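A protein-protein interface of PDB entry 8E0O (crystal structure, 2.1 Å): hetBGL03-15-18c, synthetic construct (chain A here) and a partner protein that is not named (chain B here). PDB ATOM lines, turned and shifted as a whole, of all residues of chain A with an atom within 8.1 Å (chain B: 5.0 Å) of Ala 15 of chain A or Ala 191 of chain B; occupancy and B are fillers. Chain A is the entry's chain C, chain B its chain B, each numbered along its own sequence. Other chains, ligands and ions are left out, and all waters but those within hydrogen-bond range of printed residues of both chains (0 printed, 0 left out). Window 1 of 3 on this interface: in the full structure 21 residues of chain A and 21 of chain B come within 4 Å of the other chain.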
ATOM      1  N   ALA A   8     -11.729  -6.368 -12.331  1.00  0.00           N
ATOM      2  CA  ALA A   8     -12.555  -7.483 -11.878  1.00  0.00           C
ATOM      3  C   ALA A   8     -12.628  -8.580 -12.933  1.00  0.00           C
ATOM      4  O   ALA A   8     -12.617  -9.771 -12.600  1.00  0.00           O
ATOM      5  CB  ALA A   8     -13.954  -6.987 -11.516  1.00  0.00           C
ATOM      6  N   LEU A   9     -12.701  -8.200 -14.212  1.00  0.00           N
ATOM      7  CA  LEU A   9     -12.723  -9.197 -15.276  1.00  0.00           C
ATOM      8  C   LEU A   9     -11.396  -9.937 -15.381  1.00  0.00           C
ATOM      9  O   LEU A   9     -11.377 -11.125 -15.722  1.00  0.00           O
ATOM     10  CB  LEU A   9     -13.072  -8.538 -16.609  1.00  0.00           C
ATOM     11  CG  LEU A   9     -14.458  -7.895 -16.701  1.00  0.00           C
ATOM     12  CD1 LEU A   9     -14.728  -7.407 -18.114  1.00  0.00           C
ATOM     13  CD2 LEU A   9     -15.535  -8.869 -16.246  1.00  0.00           C
ATOM     14  N   GLU A  10     -10.281  -9.257 -15.100  1.00  0.00           N
ATOM     15  CA  GLU A  10      -8.988  -9.933 -15.099  1.00  0.00           C
ATOM     16  C   GLU A  10      -8.929 -11.003 -14.018  1.00  0.00           C
ATOM     17  O   GLU A  10      -8.429 -12.108 -14.254  1.00  0.00           O
ATOM     18  CB  GLU A  10      -7.859  -8.919 -14.914  1.00  0.00           C
ATOM     19  CG  GLU A  10      -7.764  -7.890 -16.027  1.00  0.00           C
ATOM     20  CD  GLU A  10      -6.947  -6.675 -15.637  1.00  0.00           C
ATOM     21  OE1 GLU A  10      -6.438  -5.985 -16.545  1.00  0.00           O
ATOM     22  OE2 GLU A  10      -6.813  -6.409 -14.424  1.00  0.00           O
ATOM     23  N   ASN A  11      -9.433 -10.690 -12.820  1.00  0.00           N
ATOM     24  CA  ASN A  11      -9.516 -11.695 -11.764  1.00  0.00           C
ATOM     25  C   ASN A  11     -10.419 -12.846 -12.180  1.00  0.00           C
ATOM     26  O   ASN A  11     -10.134 -14.012 -11.884  1.00  0.00           O
ATOM     27  CB  ASN A  11     -10.035 -11.063 -10.472  1.00  0.00           C
ATOM     28  CG  ASN A  11      -8.983 -10.240  -9.757  1.00  0.00           C
ATOM     29  OD1 ASN A  11      -7.817 -10.227 -10.147  1.00  0.00           O
ATOM     30  ND2 ASN A  11      -9.392  -9.548  -8.699  1.00  0.00           N
ATOM     31  N   MET A  12     -11.509 -12.532 -12.880  1.00  0.00           N
ATOM     32  CA  MET A  12     -12.510 -13.537 -13.215  1.00  0.00           C
ATOM     33  C   MET A  12     -11.983 -14.524 -14.251  1.00  0.00           C
ATOM     34  O   MET A  12     -12.218 -15.734 -14.136  1.00  0.00           O
ATOM     35  CB  MET A  12     -13.773 -12.837 -13.713  1.00  0.00           C
ATOM     36  CG  MET A  12     -14.696 -12.366 -12.602  1.00  0.00           C
ATOM     37  SD  MET A  12     -16.176 -11.547 -13.225  1.00  0.00           S
ATOM     38  CE  MET A  12     -17.200 -12.955 -13.650  1.00  0.00           C
ATOM     39  N   VAL A  13     -11.270 -14.033 -15.266  1.00  0.00           N
ATOM     40  CA  VAL A  13     -10.731 -14.933 -16.281  1.00  0.00           C
ATOM     41  C   VAL A  13      -9.565 -15.741 -15.724  1.00  0.00           C
ATOM     42  O   VAL A  13      -9.342 -16.885 -16.138  1.00  0.00           O
ATOM     43  CB  VAL A  13     -10.333 -14.146 -17.545  1.00  0.00           C
ATOM     44  CG1 VAL A  13      -9.070 -13.321 -17.312  1.00  0.00           C
ATOM     45  CG2 VAL A  13     -10.146 -15.094 -18.720  1.00  0.00           C
ATOM     46  N   ARG A  14      -8.811 -15.177 -14.777  1.00  0.00           N
ATOM     47  CA  ARG A  14      -7.749 -15.944 -14.133  1.00  0.00           C
ATOM     48  C   ARG A  14      -8.332 -17.035 -13.243  1.00  0.00           C
ATOM     49  O   ARG A  14      -7.776 -18.136 -13.156  1.00  0.00           O
ATOM     50  CB  ARG A  14      -6.843 -15.015 -13.326  1.00  0.00           C
ATOM     51  N   ALA A  15      -9.455 -16.747 -12.581  1.00  0.00           N
ATOM     52  CA  ALA A  15     -10.123 -17.766 -11.780  1.00  0.00           C
ATOM     53  C   ALA A  15     -10.702 -18.866 -12.660  1.00  0.00           C
ATOM     54  O   ALA A  15     -10.672 -20.045 -12.288  1.00  0.00           O
ATOM     55  CB  ALA A  15     -11.216 -17.128 -10.923  1.00  0.00           C
ATOM     56  N   ALA A  16     -11.233 -18.502 -13.831  1.00  0.00           N
ATOM     57  CA  ALA A  16     -11.773 -19.508 -14.742  1.00  0.00           C
ATOM     58  C   ALA A  16     -10.678 -20.443 -15.237  1.00  0.00           C
ATOM     59  O   ALA A  16     -10.911 -21.645 -15.414  1.00  0.00           O
ATOM     60  CB  ALA A  16     -12.474 -18.831 -15.920  1.00  0.00           C
ATOM     61  N   HIS A  17      -9.478 -19.908 -15.470  1.00  0.00           N
ATOM     62  CA  HIS A  17      -8.351 -20.757 -15.839  1.00  0.00           C
ATOM     63  C   HIS A  17      -7.982 -21.698 -14.700  1.00  0.00           C
ATOM     64  O   HIS A  17      -7.671 -22.873 -14.929  1.00  0.00           O
ATOM     65  CB  HIS A  17      -7.153 -19.893 -16.234  1.00  0.00           C
ATOM     66  CG  HIS A  17      -6.059 -20.650 -16.917  1.00  0.00           C
ATOM     67  ND1 HIS A  17      -5.071 -21.319 -16.226  1.00  0.00           N
ATOM     68  CD2 HIS A  17      -5.794 -20.845 -18.231  1.00  0.00           C
ATOM     69  CE1 HIS A  17      -4.246 -21.892 -17.084  1.00  0.00           C
ATOM     70  NE2 HIS A  17      -4.663 -21.620 -18.308  1.00  0.00           N
ATOM     71  N   THR A  18      -8.017 -21.199 -13.462  1.00  0.00           N
ATOM     72  CA  THR A  18      -7.730 -22.050 -12.312  1.00  0.00           C
ATOM     73  C   THR A  18      -8.817 -23.101 -12.121  1.00  0.00           C
ATOM     74  O   THR A  18      -8.517 -24.266 -11.836  1.00  0.00           O
ATOM     75  CB  THR A  18      -7.579 -21.194 -11.052  1.00  0.00           C
ATOM     76  OG1 THR A  18      -6.461 -20.311 -11.204  1.00  0.00           O
ATOM     77  CG2 THR A  18      -7.359 -22.073  -9.828  1.00  0.00           C
ATOM     78  N   LEU A  19     -10.084 -22.710 -12.282  1.00  0.00           N
ATOM     79  CA  LEU A  19     -11.181 -23.665 -12.141  1.00  0.00           C
ATOM     80  C   LEU A  19     -11.073 -24.787 -13.166  1.00  0.00           C
ATOM     81  O   LEU A  19     -11.397 -25.943 -12.870  1.00  0.00           O
ATOM     82  CB  LEU A  19     -12.525 -22.947 -12.277  1.00  0.00           C
ATOM     83  CG  LEU A  19     -12.970 -22.020 -11.146  1.00  0.00           C
ATOM     84  CD1 LEU A  19     -14.339 -21.431 -11.452  1.00  0.00           C
ATOM     85  CD2 LEU A  19     -12.987 -22.754  -9.817  1.00  0.00           C
ATOM     86  N   ALA A  20     -10.624 -24.464 -14.381  1.00  0.00           N
ATOM     87  CA  ALA A  20     -10.464 -25.492 -15.405  1.00  0.00           C
ATOM     88  C   ALA A  20      -9.323 -26.439 -15.059  1.00  0.00           C
ATOM     89  O   ALA A  20      -9.405 -27.643 -15.328  1.00  0.00           O
ATOM     90  CB  ALA A  20     -10.232 -24.844 -16.769  1.00  0.00           C
ATOM     91  N   GLU A  21      -8.252 -25.914 -14.459  1.00  0.00           N
ATOM     92  CA  GLU A  21      -7.138 -26.765 -14.060  1.00  0.00           C
ATOM     93  C   GLU A  21      -7.535 -27.702 -12.928  1.00  0.00           C
ATOM     94  O   GLU A  21      -7.199 -28.891 -12.950  1.00  0.00           O
ATOM     95  CB  GLU A  21      -5.944 -25.906 -13.649  1.00  0.00           C
ATOM     96  CG  GLU A  21      -4.595 -26.571 -13.867  1.00  0.00           C
ATOM     97  CD  GLU A  21      -3.572 -25.625 -14.461  1.00  0.00           C
ATOM     98  OE1 GLU A  21      -3.539 -25.485 -15.701  1.00  0.00           O
ATOM     99  OE2 GLU A  21      -2.801 -25.020 -13.687  1.00  0.00           O
ATOM    100  N   ILE A  22      -8.250 -27.182 -11.926  1.00  0.00           N
ATOM    101  CA  ILE A  22      -8.686 -28.016 -10.809  1.00  0.00           C
ATOM    102  C   ILE A  22      -9.657 -29.083 -11.294  1.00  0.00           C
ATOM    103  O   ILE A  22      -9.648 -30.222 -10.808  1.00  0.00           O
ATOM    104  CB  ILE A  22      -9.312 -27.143  -9.704  1.00  0.00           C
ATOM    105  CG1 ILE A  22      -8.306 -26.104  -9.205  1.00  0.00           C
ATOM    106  CG2 ILE A  22      -9.785 -28.007  -8.549  1.00  0.00           C
ATOM    107  CD1 ILE A  22      -8.825 -25.255  -8.063  1.00  0.00           C
ATOM    108  N   ARG A  34     -18.459 -25.806 -15.192  1.00  0.00           N
ATOM    109  CA  ARG A  34     -18.556 -24.595 -14.387  1.00  0.00           C
ATOM    110  C   ARG A  34     -17.408 -23.637 -14.681  1.00  0.00           C
ATOM    111  O   ARG A  34     -17.577 -22.416 -14.580  1.00  0.00           O
ATOM    112  CB  ARG A  34     -18.607 -24.968 -12.903  1.00  0.00           C
ATOM    113  CG  ARG A  34     -19.976 -25.515 -12.504  1.00  0.00           C
ATOM    114  CD  ARG A  34     -20.294 -25.443 -11.014  1.00  0.00           C
ATOM    115  NE  ARG A  34     -21.062 -26.612 -10.596  1.00  0.00           N
ATOM    116  CZ  ARG A  34     -20.799 -27.353  -9.529  1.00  0.00           C
ATOM    117  NH1 ARG A  34     -19.853 -27.016  -8.670  1.00  0.00           N
ATOM    118  NH2 ARG A  34     -21.521 -28.448  -9.304  1.00  0.00           N
ATOM    119  N   ALA A  35     -16.246 -24.170 -15.063  1.00  0.00           N
ATOM    120  CA  ALA A  35     -15.132 -23.314 -15.453  1.00  0.00           C
ATOM    121  C   ALA A  35     -15.359 -22.710 -16.831  1.00  0.00           C
ATOM    122  O   ALA A  35     -15.062 -21.531 -17.054  1.00  0.00           O
ATOM    123  CB  ALA A  35     -13.827 -24.108 -15.427  1.00  0.00           C
ATOM    124  N   LEU A  38     -17.740 -19.768 -16.612  1.00  0.00           N
ATOM    125  CA  LEU A  38     -17.128 -18.522 -16.167  1.00  0.00           C
ATOM    126  C   LEU A  38     -16.327 -17.869 -17.286  1.00  0.00           C
ATOM    127  O   LEU A  38     -16.377 -16.645 -17.459  1.00  0.00           O
ATOM    128  CB  LEU A  38     -16.244 -18.780 -14.947  1.00  0.00           C
ATOM    129  CG  LEU A  38     -15.660 -17.550 -14.250  1.00  0.00           C
ATOM    130  CD1 LEU A  38     -16.771 -16.634 -13.767  1.00  0.00           C
ATOM    131  CD2 LEU A  38     -14.770 -17.970 -13.091  1.00  0.00           C
ATOM    132  N   ALA A  39     -15.585 -18.667 -18.058  1.00  0.00           N
ATOM    133  CA  ALA A  39     -14.824 -18.112 -19.173  1.00  0.00           C
ATOM    134  C   ALA A  39     -15.748 -17.502 -20.219  1.00  0.00           C
ATOM    135  O   ALA A  39     -15.445 -16.444 -20.786  1.00  0.00           O
ATOM    136  CB  ALA A  39     -13.939 -19.191 -19.795  1.00  0.00           C
ATOM    137  N   GLU A  41     -18.736 -16.241 -19.587  1.00  0.00           N
ATOM    138  CA  GLU A  41     -19.280 -15.021 -18.999  1.00  0.00           C
ATOM    139  C   GLU A  41     -18.281 -13.875 -19.087  1.00  0.00           C
ATOM    140  O   GLU A  41     -18.660 -12.730 -19.363  1.00  0.00           O
ATOM    141  CB  GLU A  41     -19.682 -15.273 -17.545  1.00  0.00           C
ATOM    142  CG  GLU A  41     -20.065 -14.012 -16.784  1.00  0.00           C
ATOM    143  CD  GLU A  41     -20.302 -14.260 -15.308  1.00  0.00           C
ATOM    144  OE1 GLU A  41     -20.322 -15.438 -14.891  1.00  0.00           O
ATOM    145  OE2 GLU A  41     -20.461 -13.270 -14.562  1.00  0.00           O
ATOM    146  N   VAL A  42     -16.998 -14.163 -18.858  1.00  0.00           N
ATOM    147  CA  VAL A  42     -15.973 -13.129 -18.970  1.00  0.00           C
ATOM    148  C   VAL A  42     -15.882 -12.623 -20.405  1.00  0.00           C
ATOM    149  O   VAL A  42     -15.723 -11.421 -20.646  1.00  0.00           O
ATOM    150  CB  VAL A  42     -14.619 -13.662 -18.469  1.00  0.00           C
ATOM    151  CG1 VAL A  42     -13.514 -12.660 -18.751  1.00  0.00           C
ATOM    152  CG2 VAL A  42     -14.690 -13.972 -16.983  1.00  0.00           C
ATOM    153  N   VAL A  75      -8.888 -19.669 -22.645  1.00  0.00           N
ATOM    154  CA  VAL A  75      -9.362 -20.631 -21.653  1.00  0.00           C
ATOM    155  C   VAL A  75     -10.413 -21.550 -22.263  1.00  0.00           C
ATOM    156  O   VAL A  75     -10.413 -22.764 -22.024  1.00  0.00           O
ATOM    157  CB  VAL A  75      -9.903 -19.897 -20.412  1.00  0.00           C
ATOM    158  CG1 VAL A  75     -10.510 -20.887 -19.429  1.00  0.00           C
ATOM    159  CG2 VAL A  75      -8.798 -19.089 -19.748  1.00  0.00           C
ATOM    160  N   ASN B 161      -6.643 -15.927  -5.489  1.00  0.00           N
ATOM    161  CA  ASN B 161      -6.675 -16.915  -6.562  1.00  0.00           C
ATOM    162  C   ASN B 161      -5.293 -17.506  -6.812  1.00  0.00           C
ATOM    163  O   ASN B 161      -5.168 -18.702  -7.103  1.00  0.00           O
ATOM    164  CB  ASN B 161      -7.226 -16.288  -7.842  1.00  0.00           C
ATOM    165  CG  ASN B 161      -7.218 -17.252  -9.011  1.00  0.00           C
ATOM    166  OD1 ASN B 161      -7.948 -18.242  -9.019  1.00  0.00           O
ATOM    167  ND2 ASN B 161      -6.383 -16.971 -10.004  1.00  0.00           N
ATOM    168  N   THR B 187     -11.045 -20.271  -4.993  1.00  0.00           N
ATOM    169  CA  THR B 187     -11.097 -19.766  -6.361  1.00  0.00           C
ATOM    170  C   THR B 187     -12.494 -19.270  -6.708  1.00  0.00           C
ATOM    171  O   THR B 187     -12.647 -18.224  -7.350  1.00  0.00           O
ATOM    172  CB  THR B 187     -10.654 -20.850  -7.343  1.00  0.00           C
ATOM    173  OG1 THR B 187      -9.384 -21.374  -6.937  1.00  0.00           O
ATOM    174  CG2 THR B 187     -10.528 -20.273  -8.746  1.00  0.00           C
ATOM    175  N   HIS B 188     -13.527 -20.010  -6.291  1.00  0.00           N
ATOM    176  CA  HIS B 188     -14.895 -19.559  -6.514  1.00  0.00           C
ATOM    177  C   HIS B 188     -15.168 -18.250  -5.785  1.00  0.00           C
ATOM    178  O   HIS B 188     -15.834 -17.359  -6.324  1.00  0.00           O
ATOM    179  CB  HIS B 188     -15.884 -20.635  -6.066  1.00  0.00           C
ATOM    180  CG  HIS B 188     -16.316 -21.554  -7.166  1.00  0.00           C
ATOM    181  ND1 HIS B 188     -17.070 -21.127  -8.237  1.00  0.00           N
ATOM    182  CD2 HIS B 188     -16.102 -22.877  -7.359  1.00  0.00           C
ATOM    183  CE1 HIS B 188     -17.301 -22.147  -9.045  1.00  0.00           C
ATOM    184  NE2 HIS B 188     -16.724 -23.221  -8.535  1.00  0.00           N
ATOM    185  N   ARG B 189     -14.658 -18.116  -4.558  1.00  0.00           N
ATOM    186  CA  ARG B 189     -14.860 -16.884  -3.803  1.00  0.00           C
ATOM    187  C   ARG B 189     -14.179 -15.704  -4.483  1.00  0.00           C
ATOM    188  O   ARG B 189     -14.737 -14.602  -4.536  1.00  0.00           O
ATOM    189  CB  ARG B 189     -14.345 -17.053  -2.375  1.00  0.00           C
ATOM    190  CG  ARG B 189     -14.641 -15.873  -1.465  1.00  0.00           C
ATOM    191  CD  ARG B 189     -14.729 -16.308  -0.011  1.00  0.00           C
ATOM    192  NE  ARG B 189     -16.104 -16.316   0.472  1.00  0.00           N
ATOM    193  CZ  ARG B 189     -16.448 -16.458   1.745  1.00  0.00           C
ATOM    194  NH1 ARG B 189     -15.540 -16.608   2.695  1.00  0.00           N
ATOM    195  NH2 ARG B 189     -17.738 -16.449   2.073  1.00  0.00           N
ATOM    196  N   SER B 190     -12.970 -15.917  -5.008  1.00  0.00           N
ATOM    197  CA  SER B 190     -12.278 -14.849  -5.723  1.00  0.00           C
ATOM    198  C   SER B 190     -13.073 -14.401  -6.942  1.00  0.00           C
ATOM    199  O   SER B 190     -13.202 -13.198  -7.201  1.00  0.00           O
ATOM    200  CB  SER B 190     -10.880 -15.314  -6.130  1.00  0.00           C
ATOM    201  OG  SER B 190     -10.315 -14.448  -7.100  1.00  0.00           O
ATOM    202  N   ALA B 191     -13.628 -15.353  -7.694  1.00  0.00           N
ATOM    203  CA  ALA B 191     -14.419 -15.001  -8.868  1.00  0.00           C
ATOM    204  C   ALA B 191     -15.760 -14.393  -8.475  1.00  0.00           C
ATOM    205  O   ALA B 191     -16.227 -13.441  -9.112  1.00  0.00           O
ATOM    206  CB  ALA B 191     -14.627 -16.232  -9.749  1.00  0.00           C
ATOM    207  N   LYS B 192     -16.396 -14.928  -7.428  1.00  0.00           N
ATOM    208  CA  LYS B 192     -17.709 -14.438  -7.019  1.00  0.00           C
ATOM    209  C   LYS B 192     -17.633 -12.999  -6.521  1.00  0.00           C
ATOM    210  O   LYS B 192     -18.411 -12.142  -6.954  1.00  0.00           O
ATOM    211  CB  LYS B 192     -18.296 -15.352  -5.942  1.00  0.00           C
ATOM    212  CG  LYS B 192     -19.743 -15.050  -5.584  1.00  0.00           C
ATOM    213  CD  LYS B 192     -19.919 -14.938  -4.077  1.00  0.00           C
ATOM    214  CE  LYS B 192     -21.388 -14.860  -3.692  1.00  0.00           C
ATOM    215  NZ  LYS B 192     -22.188 -15.966  -4.284  1.00  0.00           N
ATOM    216  N   TRP B 193     -16.701 -12.716  -5.607  1.00  0.00           N
ATOM    217  CA  TRP B 193     -16.573 -11.361  -5.084  1.00  0.00           C
ATOM    218  C   TRP B 193     -16.104 -10.386  -6.155  1.00  0.00           C
ATOM    219  O   TRP B 193     -16.449  -9.200  -6.105  1.00  0.00           O
ATOM    220  CB  TRP B 193     -15.616 -11.345  -3.890  1.00  0.00           C
ATOM    221  CG  TRP B 193     -16.188 -11.976  -2.652  1.00  0.00           C
ATOM    222  CD1 TRP B 193     -17.364 -12.660  -2.549  1.00  0.00           C
ATOM    223  CD2 TRP B 193     -15.605 -11.981  -1.342  1.00  0.00           C
ATOM    224  NE1 TRP B 193     -17.551 -13.088  -1.258  1.00  0.00           N
ATOM    225  CE2 TRP B 193     -16.486 -12.686  -0.497  1.00  0.00           C
ATOM    226  CE3 TRP B 193     -14.425 -11.458  -0.803  1.00  0.00           C
ATOM    227  CZ2 TRP B 193     -16.224 -12.880   0.859  1.00  0.00           C
ATOM    228  CZ3 TRP B 193     -14.168 -11.653   0.544  1.00  0.00           C
ATOM    229  CH2 TRP B 193     -15.063 -12.358   1.358  1.00  0.00           C
ATOM    230  N   SER B 194     -15.322 -10.861  -7.129  1.00  0.00           N
ATOM    231  CA  SER B 194     -14.889  -9.987  -8.214  1.00  0.00           C
ATOM    232  C   SER B 194     -16.058  -9.612  -9.118  1.00  0.00           C
ATOM    233  O   SER B 194     -16.155  -8.464  -9.569  1.00  0.00           O
ATOM    234  CB  SER B 194     -13.780 -10.661  -9.022  1.00  0.00           C
ATOM    235  OG  SER B 194     -12.605 -10.816  -8.244  1.00  0.00           O
ATOM    236  N   ARG B 195     -16.954 -10.564  -9.394  1.00  0.00           N
ATOM    237  CA  ARG B 195     -18.139 -10.248 -10.184  1.00  0.00           C
ATOM    238  C   ARG B 195     -19.028  -9.244  -9.461  1.00  0.00           C
ATOM    239  O   ARG B 195     -19.603  -8.348 -10.089  1.00  0.00           O
ATOM    240  CB  ARG B 195     -18.927 -11.521 -10.502  1.00  0.00           C
ATOM    241  CG  ARG B 195     -20.156 -11.263 -11.367  1.00  0.00           C
ATOM    242  CD  ARG B 195     -21.149 -12.418 -11.331  1.00  0.00           C
ATOM    243  NE  ARG B 195     -20.642 -13.609 -12.002  1.00  0.00           N
ATOM    244  CZ  ARG B 195     -20.314 -14.734 -11.382  1.00  0.00           C
ATOM    245  NH1 ARG B 195     -20.433 -14.860 -10.070  1.00  0.00           N
ATOM    246  NH2 ARG B 195     -19.862 -15.760 -12.097  1.00  0.00           N
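The guanidinium group of Arg 195 of chain B is in salt-bridge range of the side-chain carboxylate of Glu 41 of chain A (2.6 Å). The side-chain amide oxygen (OD1) of Asn 161 of chain B is in hydrogen-bond range of the side-chain hydroxyl (OG1) of Thr 18 of chain A (3.4 Å). The side-chain hydroxyl (OG) of Ser 194 of chain B sits close to the side-chain amide nitrogen (ND2) of Asn 11 of chain A, at 3.5 Å.
Ala 15 of chain A touches just these residues of chain B: Asn 161, Thr 187 and Ala 191. Of chain A, only Met 12, Ala 15 and Leu 38 come within 4 Å of Ala 191 of chain B. No residue of chain A comes within 4 Å of Ser 190 of chain B. Printed residues of chain B within 4 Å of Ala 8 of chain A: Ser 194 (3.3 Å). Of the printed residues of chain A, His 188 of chain B touches Leu 19. Printed residues of chain B within 4 Å of Thr 18 of chain A: Asn 161 (3.4 Å) and Thr 187 (3.6 Å). Of the printed residues of chain A, Asn 161 of chain B touches Arg 14, Ala 15 and Thr 18. Of the printed residues of chain B, Met 12 of chain A touches Ala 191 and Arg 195. The nearest residue of chain A that does not touch Ala 191 of chain B is Asn 11 of chain A (5.3 Å).
Among the printed residues, pairs that only touch across the chains: Ala 8 of chain A with Ser 194 of chain B (3.3 Å), Met 12 of chain A with Ala 191 of chain B (3.96 Å), Met 12 of chain A with Arg 195 of chain B (3.8 Å), Arg 14 of chain A with Asn 161 of chain B (3.6 Å), Ala 15 of chain A with Asn 161 of chain B (3.5 Å), Ala 15 of chain A with Thr 187 of chain B (3.6 Å), Ala 15 of chain A with Ala 191 of chain B (3.7 Å), Thr 18 of chain A with Thr 187 of chain B (3.6 Å), Leu 19 of chain A with Thr 187 of chain B (3.7 Å), Leu 19 of chain A with His 188 of chain B (3.9 Å), Leu 38 of chain A with Ala 191 of chain B (3.8 Å) and Leu 38 of chain A with Arg 195 of chain B (3.6 Å).
OG of Ser 194 of chain B is in hydrogen-bond range of O of Ser 190 of chain B, at 2.7 Å. O of Arg 14 of chain A lies within hydrogen-bond range of OG1 of Thr 18 of chain A (3.2 Å).
Printed residues of chain A that touch a printed residue of chain B: Ala 8, Asn 11, Met 12, Arg 14, Ala 15, Thr 18, Leu 19, Leu 38 and Glu 41. Along chain A the printed residues that touch a printed residue of chain B span positions 8 to 41. Of the 10 printed residues of chain B, 6 touch a printed residue of chain A. Hydrophobic or aromatic side chains of chain B that line the printed part of chain A: His 188 and Ala 191. Among the printed residues, 15 pairs touch across the chains. Among the printed residues, Asp or Glu carboxylates within 4 Å of a Lys or Arg side-chain nitrogen of the other chain: Glu 41 of chain A with Arg 195 of chain B.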
